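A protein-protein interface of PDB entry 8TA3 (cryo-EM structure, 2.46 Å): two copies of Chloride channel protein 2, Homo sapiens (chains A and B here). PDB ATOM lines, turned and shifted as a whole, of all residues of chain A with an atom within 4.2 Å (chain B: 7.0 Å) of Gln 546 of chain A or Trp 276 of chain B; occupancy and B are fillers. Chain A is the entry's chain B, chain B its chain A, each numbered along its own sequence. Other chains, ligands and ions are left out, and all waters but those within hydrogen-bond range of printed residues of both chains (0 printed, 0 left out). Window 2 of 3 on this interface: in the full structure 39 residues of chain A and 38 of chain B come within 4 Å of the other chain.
Printed residues of chain A that touch a printed residue of chain B: Glu 264, His 513, Val 515 and Gln 546.
Of the 15 printed residues of chain B, 3 touch a printed residue of chain A.
Printed residues of chain B that touch a printed residue of chain A: Tyr 275, Trp 276 and Phe 279.
Hydrophobic or aromatic side chains of chain B within 4 Å of the printed part of chain A: Tyr 275, Trp 276 and Phe 279.
Among the printed residues, 7 pairs touch across the chains.
No position is printed for both chains.
Of the 7 pairs that touch across the chains among the printed residues, none has its exchanged pair printed and touching as well.
OE1 of Glu 264 of chain A lies within hydrogen-bond range of NE1 of Trp 276 of chain B, 2.8 Å away.
The backbone NH (N) of Val 515 of chain A sits at hydrogen-bond distance from the side-chain carboxylate (OE1) of Glu 264 of chain A.
NE2 of His 513 of chain A is in hydrogen-bond range of O of Gln 549 of chain A, 2.9 Å away.
Among the printed residues, merely in contact across the chains: Glu 264 of chain A with Tyr 275 of chain B (3.7 Å), His 513 of chain A with Trp 276 of chain B (3.4 Å), Val 515 of chain A with Tyr 275 of chain B (3.6 Å), Val 515 of chain A with Trp 276 of chain B (3.9 Å), Val 515 of chain A with Phe 279 of chain B (3.8 Å) and Gln 546 of chain A with Trp 276 of chain B (3.6 Å).
Of chain B, only Trp 276 comes within 4 Å of Gln 546 of chain A.
Of chain A, only Glu 264, His 513, Val 515 and Gln 546 come within 4 Å of Trp 276 of chain B.
Printed residues of chain B within 4 Å of His 513 of chain A: Trp 276.
Of the printed residues of chain B, Glu 264 of chain A touches Tyr 275 (3.7 Å) and Trp 276 (2.8 Å).
Of the printed residues of chain B, Val 515 of chain A touches Tyr 275 (3.6 Å), Trp 276 (3.9 Å) and Phe 279 (3.8 Å).
Of the printed residues of chain A, Phe 279 of chain B touches Val 515 (3.8 Å).
The nearest printed residue of chain B that does not touch Gln 546 of chain A is Arg 273 of chain B (7.2 Å).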
ATOM      1  N   GLU A 264      22.433 -11.940   6.330  1.00  0.00           N
ATOM      2  CA  GLU A 264      22.726 -13.240   6.941  1.00  0.00           C
ATOM      3  C   GLU A 264      21.625 -13.753   7.879  1.00  0.00           C
ATOM      4  O   GLU A 264      21.420 -14.960   7.951  1.00  0.00           O
ATOM      5  CB  GLU A 264      24.039 -13.189   7.736  1.00  0.00           C
ATOM      6  CG  GLU A 264      25.300 -13.142   6.879  1.00  0.00           C
ATOM      7  CD  GLU A 264      26.547 -13.376   7.745  1.00  0.00           C
ATOM      8  OE1 GLU A 264      26.883 -14.537   8.051  1.00  0.00           O
ATOM      9  OE2 GLU A 264      27.212 -12.393   8.129  1.00  0.00           O
ATOM     10  N   HIS A 513      25.240 -17.015  14.484  1.00  0.00           N
ATOM     11  CA  HIS A 513      25.732 -17.719  13.284  1.00  0.00           C
ATOM     12  C   HIS A 513      25.998 -16.764  12.115  1.00  0.00           C
ATOM     13  O   HIS A 513      25.502 -16.966  11.016  1.00  0.00           O
ATOM     14  CB  HIS A 513      24.861 -18.924  12.875  1.00  0.00           C
ATOM     15  CG  HIS A 513      24.845 -20.091  13.821  1.00  0.00           C
ATOM     16  ND1 HIS A 513      25.487 -20.154  15.050  1.00  0.00           N
ATOM     17  CD2 HIS A 513      24.249 -21.290  13.575  1.00  0.00           C
ATOM     18  CE1 HIS A 513      25.270 -21.387  15.522  1.00  0.00           C
ATOM     19  NE2 HIS A 513      24.541 -22.096  14.650  1.00  0.00           N
ATOM     20  N   VAL A 515      29.165 -14.188  10.029  1.00  0.00           N
ATOM     21  CA  VAL A 515      30.561 -13.733   9.857  1.00  0.00           C
ATOM     22  C   VAL A 515      30.676 -12.211   9.795  1.00  0.00           C
ATOM     23  O   VAL A 515      31.726 -11.659  10.097  1.00  0.00           O
ATOM     24  CB  VAL A 515      31.273 -14.384   8.655  1.00  0.00           C
ATOM     25  CG1 VAL A 515      31.340 -15.901   8.801  1.00  0.00           C
ATOM     26  CG2 VAL A 515      30.652 -14.028   7.306  1.00  0.00           C
ATOM     27  N   ASN A 542      32.373 -19.691  14.377  1.00  0.00           N
ATOM     28  CA  ASN A 542      31.294 -20.220  13.537  1.00  0.00           C
ATOM     29  C   ASN A 542      31.429 -21.718  13.230  1.00  0.00           C
ATOM     30  O   ASN A 542      30.458 -22.451  13.384  1.00  0.00           O
ATOM     31  CB  ASN A 542      31.209 -19.415  12.238  1.00  0.00           C
ATOM     32  CG  ASN A 542      30.355 -18.181  12.397  1.00  0.00           C
ATOM     33  OD1 ASN A 542      29.147 -18.251  12.294  1.00  0.00           O
ATOM     34  ND2 ASN A 542      30.930 -17.033  12.643  1.00  0.00           N
ATOM     35  N   VAL A 544      32.960 -24.131  14.938  1.00  0.00           N
ATOM     36  CA  VAL A 544      32.654 -24.859  16.179  1.00  0.00           C
ATOM     37  C   VAL A 544      31.173 -24.737  16.581  1.00  0.00           C
ATOM     38  O   VAL A 544      30.557 -25.752  16.887  1.00  0.00           O
ATOM     39  CB  VAL A 544      33.602 -24.421  17.313  1.00  0.00           C
ATOM     40  CG1 VAL A 544      33.208 -24.971  18.682  1.00  0.00           C
ATOM     41  CG2 VAL A 544      35.029 -24.899  17.039  1.00  0.00           C
ATOM     42  N   ALA A 545      30.559 -23.550  16.556  1.00  0.00           N
ATOM     43  CA  ALA A 545      29.186 -23.361  17.040  1.00  0.00           C
ATOM     44  C   ALA A 545      28.111 -24.058  16.186  1.00  0.00           C
ATOM     45  O   ALA A 545      27.217 -24.706  16.727  1.00  0.00           O
ATOM     46  CB  ALA A 545      28.890 -21.865  17.155  1.00  0.00           C
ATOM     47  N   GLN A 546      28.198 -23.973  14.854  1.00  0.00           N
ATOM     48  CA  GLN A 546      27.238 -24.589  13.931  1.00  0.00           C
ATOM     49  C   GLN A 546      27.203 -26.125  14.017  1.00  0.00           C
ATOM     50  O   GLN A 546      26.204 -26.747  13.667  1.00  0.00           O
ATOM     51  CB  GLN A 546      27.551 -24.151  12.498  1.00  0.00           C
ATOM     52  CG  GLN A 546      27.283 -22.661  12.279  1.00  0.00           C
ATOM     53  CD  GLN A 546      27.542 -22.192  10.858  1.00  0.00           C
ATOM     54  OE1 GLN A 546      27.694 -22.974   9.934  1.00  0.00           O
ATOM     55  NE2 GLN A 546      27.578 -20.902  10.615  1.00  0.00           N
ATOM     56  N   SER A 547      28.272 -26.747  14.503  1.00  0.00           N
ATOM     57  CA  SER A 547      28.363 -28.187  14.758  1.00  0.00           C
ATOM     58  C   SER A 547      27.600 -28.628  16.022  1.00  0.00           C
ATOM     59  O   SER A 547      27.283 -29.806  16.192  1.00  0.00           O
ATOM     60  CB  SER A 547      29.855 -28.526  14.853  1.00  0.00           C
ATOM     61  OG  SER A 547      30.076 -29.908  15.002  1.00  0.00           O
ATOM     62  N   LEU A 548      27.283 -27.688  16.919  1.00  0.00           N
ATOM     63  CA  LEU A 548      26.697 -27.943  18.236  1.00  0.00           C
ATOM     64  C   LEU A 548      25.226 -27.511  18.357  1.00  0.00           C
ATOM     65  O   LEU A 548      24.437 -28.240  18.954  1.00  0.00           O
ATOM     66  CB  LEU A 548      27.559 -27.239  19.305  1.00  0.00           C
ATOM     67  CG  LEU A 548      29.004 -27.753  19.436  1.00  0.00           C
ATOM     68  CD1 LEU A 548      29.799 -26.833  20.360  1.00  0.00           C
ATOM     69  CD2 LEU A 548      29.062 -29.165  20.015  1.00  0.00           C
ATOM     70  N   GLN A 549      24.841 -26.342  17.833  1.00  0.00           N
ATOM     71  CA  GLN A 549      23.525 -25.720  18.041  1.00  0.00           C
ATOM     72  C   GLN A 549      23.019 -24.935  16.812  1.00  0.00           C
ATOM     73  O   GLN A 549      23.823 -24.515  15.980  1.00  0.00           O
ATOM     74  CB  GLN A 549      23.580 -24.760  19.250  1.00  0.00           C
ATOM     75  CG  GLN A 549      23.647 -25.434  20.626  1.00  0.00           C
ATOM     76  CD  GLN A 549      22.395 -26.226  20.978  1.00  0.00           C
ATOM     77  OE1 GLN A 549      21.347 -25.688  21.304  1.00  0.00           O
ATOM     78  NE2 GLN A 549      22.445 -27.531  20.916  1.00  0.00           N
ATOM     79  N   LEU B  94      38.678 -26.279   0.666  1.00  0.00           N
ATOM     80  CA  LEU B  94      38.837 -24.836   0.852  1.00  0.00           C
ATOM     81  C   LEU B  94      40.195 -24.442   1.463  1.00  0.00           C
ATOM     82  O   LEU B  94      40.700 -23.366   1.147  1.00  0.00           O
ATOM     83  CB  LEU B  94      37.672 -24.294   1.694  1.00  0.00           C
ATOM     84  CG  LEU B  94      36.283 -24.366   1.033  1.00  0.00           C
ATOM     85  CD1 LEU B  94      35.213 -24.013   2.062  1.00  0.00           C
ATOM     86  CD2 LEU B  94      36.113 -23.416  -0.149  1.00  0.00           C
ATOM     87  N   VAL B 259      35.637 -11.094  -1.581  1.00  0.00           N
ATOM     88  CA  VAL B 259      34.479 -11.995  -1.488  1.00  0.00           C
ATOM     89  C   VAL B 259      33.205 -11.268  -1.917  1.00  0.00           C
ATOM     90  O   VAL B 259      32.519 -11.737  -2.819  1.00  0.00           O
ATOM     91  CB  VAL B 259      34.334 -12.592  -0.074  1.00  0.00           C
ATOM     92  CG1 VAL B 259      33.098 -13.483   0.058  1.00  0.00           C
ATOM     93  CG2 VAL B 259      35.535 -13.443   0.327  1.00  0.00           C
ATOM     94  N   ILE B 263      30.787 -11.794  -5.632  1.00  0.00           N
ATOM     95  CA  ILE B 263      29.341 -12.038  -5.578  1.00  0.00           C
ATOM     96  C   ILE B 263      28.582 -11.041  -6.461  1.00  0.00           C
ATOM     97  O   ILE B 263      27.722 -11.466  -7.224  1.00  0.00           O
ATOM     98  CB  ILE B 263      28.844 -12.019  -4.113  1.00  0.00           C
ATOM     99  CG1 ILE B 263      29.424 -13.227  -3.349  1.00  0.00           C
ATOM    100  CG2 ILE B 263      27.308 -12.015  -4.021  1.00  0.00           C
ATOM    101  CD1 ILE B 263      29.227 -13.183  -1.833  1.00  0.00           C
ATOM    102  N   PHE B 270      22.885 -15.116  -4.478  1.00  0.00           N
ATOM    103  CA  PHE B 270      23.930 -15.954  -3.883  1.00  0.00           C
ATOM    104  C   PHE B 270      23.482 -16.493  -2.524  1.00  0.00           C
ATOM    105  O   PHE B 270      22.903 -15.758  -1.725  1.00  0.00           O
ATOM    106  CB  PHE B 270      25.211 -15.121  -3.780  1.00  0.00           C
ATOM    107  CG  PHE B 270      26.502 -15.910  -3.760  1.00  0.00           C
ATOM    108  CD1 PHE B 270      26.996 -16.444  -4.960  1.00  0.00           C
ATOM    109  CD2 PHE B 270      27.274 -16.008  -2.589  1.00  0.00           C
ATOM    110  CE1 PHE B 270      28.264 -17.045  -5.002  1.00  0.00           C
ATOM    111  CE2 PHE B 270      28.548 -16.598  -2.637  1.00  0.00           C
ATOM    112  CZ  PHE B 270      29.046 -17.115  -3.840  1.00  0.00           C
ATOM    113  N   ALA B 271      23.738 -17.770  -2.246  1.00  0.00           N
ATOM    114  CA  ALA B 271      23.431 -18.328  -0.940  1.00  0.00           C
ATOM    115  C   ALA B 271      24.327 -17.706   0.143  1.00  0.00           C
ATOM    116  O   ALA B 271      25.532 -17.543  -0.051  1.00  0.00           O
ATOM    117  CB  ALA B 271      23.568 -19.852  -0.980  1.00  0.00           C
ATOM    118  N   VAL B 272      23.776 -17.463   1.332  1.00  0.00           N
ATOM    119  CA  VAL B 272      24.556 -17.096   2.525  1.00  0.00           C
ATOM    120  C   VAL B 272      25.622 -18.161   2.829  1.00  0.00           C
ATOM    121  O   VAL B 272      26.757 -17.843   3.172  1.00  0.00           O
ATOM    122  CB  VAL B 272      23.595 -16.870   3.709  1.00  0.00           C
ATOM    123  CG1 VAL B 272      24.301 -16.726   5.054  1.00  0.00           C
ATOM    124  CG2 VAL B 272      22.765 -15.610   3.475  1.00  0.00           C
ATOM    125  N   ARG B 273      25.311 -19.437   2.578  1.00  0.00           N
ATOM    126  CA  ARG B 273      26.232 -20.570   2.747  1.00  0.00           C
ATOM    127  C   ARG B 273      27.483 -20.490   1.861  1.00  0.00           C
ATOM    128  O   ARG B 273      28.553 -20.912   2.285  1.00  0.00           O
ATOM    129  CB  ARG B 273      25.434 -21.864   2.533  1.00  0.00           C
ATOM    130  CG  ARG B 273      26.216 -23.133   2.864  1.00  0.00           C
ATOM    131  CD  ARG B 273      25.328 -24.384   2.764  1.00  0.00           C
ATOM    132  NE  ARG B 273      25.978 -25.481   2.023  1.00  0.00           N
ATOM    133  CZ  ARG B 273      26.149 -25.540   0.713  1.00  0.00           C
ATOM    134  NH1 ARG B 273      26.777 -26.532   0.165  1.00  0.00           N
ATOM    135  NH2 ARG B 273      25.700 -24.612  -0.076  1.00  0.00           N
ATOM    136  N   ASN B 274      27.404 -19.917   0.661  1.00  0.00           N
ATOM    137  CA  ASN B 274      28.585 -19.708  -0.183  1.00  0.00           C
ATOM    138  C   ASN B 274      29.369 -18.435   0.178  1.00  0.00           C
ATOM    139  O   ASN B 274      30.585 -18.414  -0.002  1.00  0.00           O
ATOM    140  CB  ASN B 274      28.212 -19.803  -1.677  1.00  0.00           C
ATOM    141  CG  ASN B 274      28.043 -21.247  -2.126  1.00  0.00           C
ATOM    142  OD1 ASN B 274      28.910 -22.082  -1.920  1.00  0.00           O
ATOM    143  ND2 ASN B 274      26.929 -21.589  -2.724  1.00  0.00           N
ATOM    144  N   TYR B 275      28.738 -17.411   0.763  1.00  0.00           N
ATOM    145  CA  TYR B 275      29.438 -16.271   1.372  1.00  0.00           C
ATOM    146  C   TYR B 275      30.337 -16.718   2.540  1.00  0.00           C
ATOM    147  O   TYR B 275      31.473 -16.265   2.646  1.00  0.00           O
ATOM    148  CB  TYR B 275      28.395 -15.206   1.772  1.00  0.00           C
ATOM    149  CG  TYR B 275      28.846 -14.080   2.689  1.00  0.00           C
ATOM    150  CD1 TYR B 275      29.927 -13.252   2.331  1.00  0.00           C
ATOM    151  CD2 TYR B 275      28.145 -13.826   3.886  1.00  0.00           C
ATOM    152  CE1 TYR B 275      30.314 -12.184   3.163  1.00  0.00           C
ATOM    153  CE2 TYR B 275      28.520 -12.749   4.708  1.00  0.00           C
ATOM    154  CZ  TYR B 275      29.604 -11.923   4.352  1.00  0.00           C
ATOM    155  OH  TYR B 275      29.962 -10.888   5.158  1.00  0.00           O
ATOM    156  N   TRP B 276      29.904 -17.697   3.340  1.00  0.00           N
ATOM    157  CA  TRP B 276      30.737 -18.324   4.368  1.00  0.00           C
ATOM    158  C   TRP B 276      31.912 -19.137   3.803  1.00  0.00           C
ATOM    159  O   TRP B 276      33.019 -19.066   4.328  1.00  0.00           O
ATOM    160  CB  TRP B 276      29.864 -19.221   5.257  1.00  0.00           C
ATOM    161  CG  TRP B 276      28.747 -18.572   6.015  1.00  0.00           C
ATOM    162  CD1 TRP B 276      28.635 -17.260   6.318  1.00  0.00           C
ATOM    163  CD2 TRP B 276      27.596 -19.215   6.642  1.00  0.00           C
ATOM    164  NE1 TRP B 276      27.514 -17.051   7.091  1.00  0.00           N
ATOM    165  CE2 TRP B 276      26.840 -18.225   7.329  1.00  0.00           C
ATOM    166  CE3 TRP B 276      27.116 -20.543   6.697  1.00  0.00           C
ATOM    167  CZ2 TRP B 276      25.677 -18.535   8.047  1.00  0.00           C
ATOM    168  CZ3 TRP B 276      25.945 -20.865   7.408  1.00  0.00           C
ATOM    169  CH2 TRP B 276      25.233 -19.866   8.092  1.00  0.00           C
ATOM    170  N   ARG B 277      31.707 -19.886   2.716  1.00  0.00           N
ATOM    171  CA  ARG B 277      32.761 -20.680   2.060  1.00  0.00           C
ATOM    172  C   ARG B 277      33.836 -19.806   1.411  1.00  0.00           C
ATOM    173  O   ARG B 277      35.015 -20.113   1.534  1.00  0.00           O
ATOM    174  CB  ARG B 277      32.139 -21.667   1.056  1.00  0.00           C
ATOM    175  CG  ARG B 277      31.366 -22.765   1.806  1.00  0.00           C
ATOM    176  CD  ARG B 277      30.551 -23.696   0.908  1.00  0.00           C
ATOM    177  NE  ARG B 277      31.409 -24.644   0.180  1.00  0.00           N
ATOM    178  CZ  ARG B 277      31.774 -24.597  -1.085  1.00  0.00           C
ATOM    179  NH1 ARG B 277      32.604 -25.483  -1.540  1.00  0.00           N
ATOM    180  NH2 ARG B 277      31.335 -23.681  -1.897  1.00  0.00           N
ATOM    181  N   GLY B 278      33.454 -18.680   0.813  1.00  0.00           N
ATOM    182  CA  GLY B 278      34.385 -17.679   0.300  1.00  0.00           C
ATOM    183  C   GLY B 278      35.204 -17.009   1.397  1.00  0.00           C
ATOM    184  O   GLY B 278      36.425 -16.956   1.299  1.00  0.00           O
ATOM    185  N   PHE B 279      34.564 -16.563   2.480  1.00  0.00           N
ATOM    186  CA  PHE B 279      35.213 -15.945   3.642  1.00  0.00           C
ATOM    187  C   PHE B 279      36.203 -16.896   4.340  1.00  0.00           C
ATOM    188  O   PHE B 279      37.303 -16.481   4.702  1.00  0.00           O
ATOM    189  CB  PHE B 279      34.098 -15.440   4.573  1.00  0.00           C
ATOM    190  CG  PHE B 279      34.480 -14.485   5.692  1.00  0.00           C
ATOM    191  CD1 PHE B 279      35.224 -14.923   6.802  1.00  0.00           C
ATOM    192  CD2 PHE B 279      34.013 -13.158   5.662  1.00  0.00           C
ATOM    193  CE1 PHE B 279      35.502 -14.052   7.867  1.00  0.00           C
ATOM    194  CE2 PHE B 279      34.275 -12.289   6.738  1.00  0.00           C
ATOM    195  CZ  PHE B 279      35.022 -12.736   7.841  1.00  0.00           C
ATOM    196  N   PHE B 280      35.875 -18.182   4.481  1.00  0.00           N
ATOM    197  CA  PHE B 280      36.787 -19.206   4.993  1.00  0.00           C
ATOM    198  C   PHE B 280      38.060 -19.342   4.145  1.00  0.00           C
ATOM    199  O   PHE B 280      39.167 -19.226   4.669  1.00  0.00           O
ATOM    200  CB  PHE B 280      36.047 -20.552   5.094  1.00  0.00           C
ATOM    201  CG  PHE B 280      36.866 -21.692   5.675  1.00  0.00           C
ATOM    202  CD1 PHE B 280      37.834 -22.350   4.896  1.00  0.00           C
ATOM    203  CD2 PHE B 280      36.673 -22.106   7.002  1.00  0.00           C
ATOM    204  CE1 PHE B 280      38.629 -23.368   5.447  1.00  0.00           C
ATOM    205  CE2 PHE B 280      37.461 -23.128   7.553  1.00  0.00           C
ATOM    206  CZ  PHE B 280      38.450 -23.754   6.782  1.00  0.00           C
ATOM    207  N   ALA B 281      37.932 -19.566   2.833  1.00  0.00           N
ATOM    208  CA  ALA B 281      39.078 -19.793   1.951  1.00  0.00           C
ATOM    209  C   ALA B 281      39.962 -18.547   1.775  1.00  0.00           C
ATOM    210  O   ALA B 281      41.183 -18.659   1.808  1.00  0.00           O
ATOM    211  CB  ALA B 281      38.563 -20.320   0.617  1.00  0.00           C
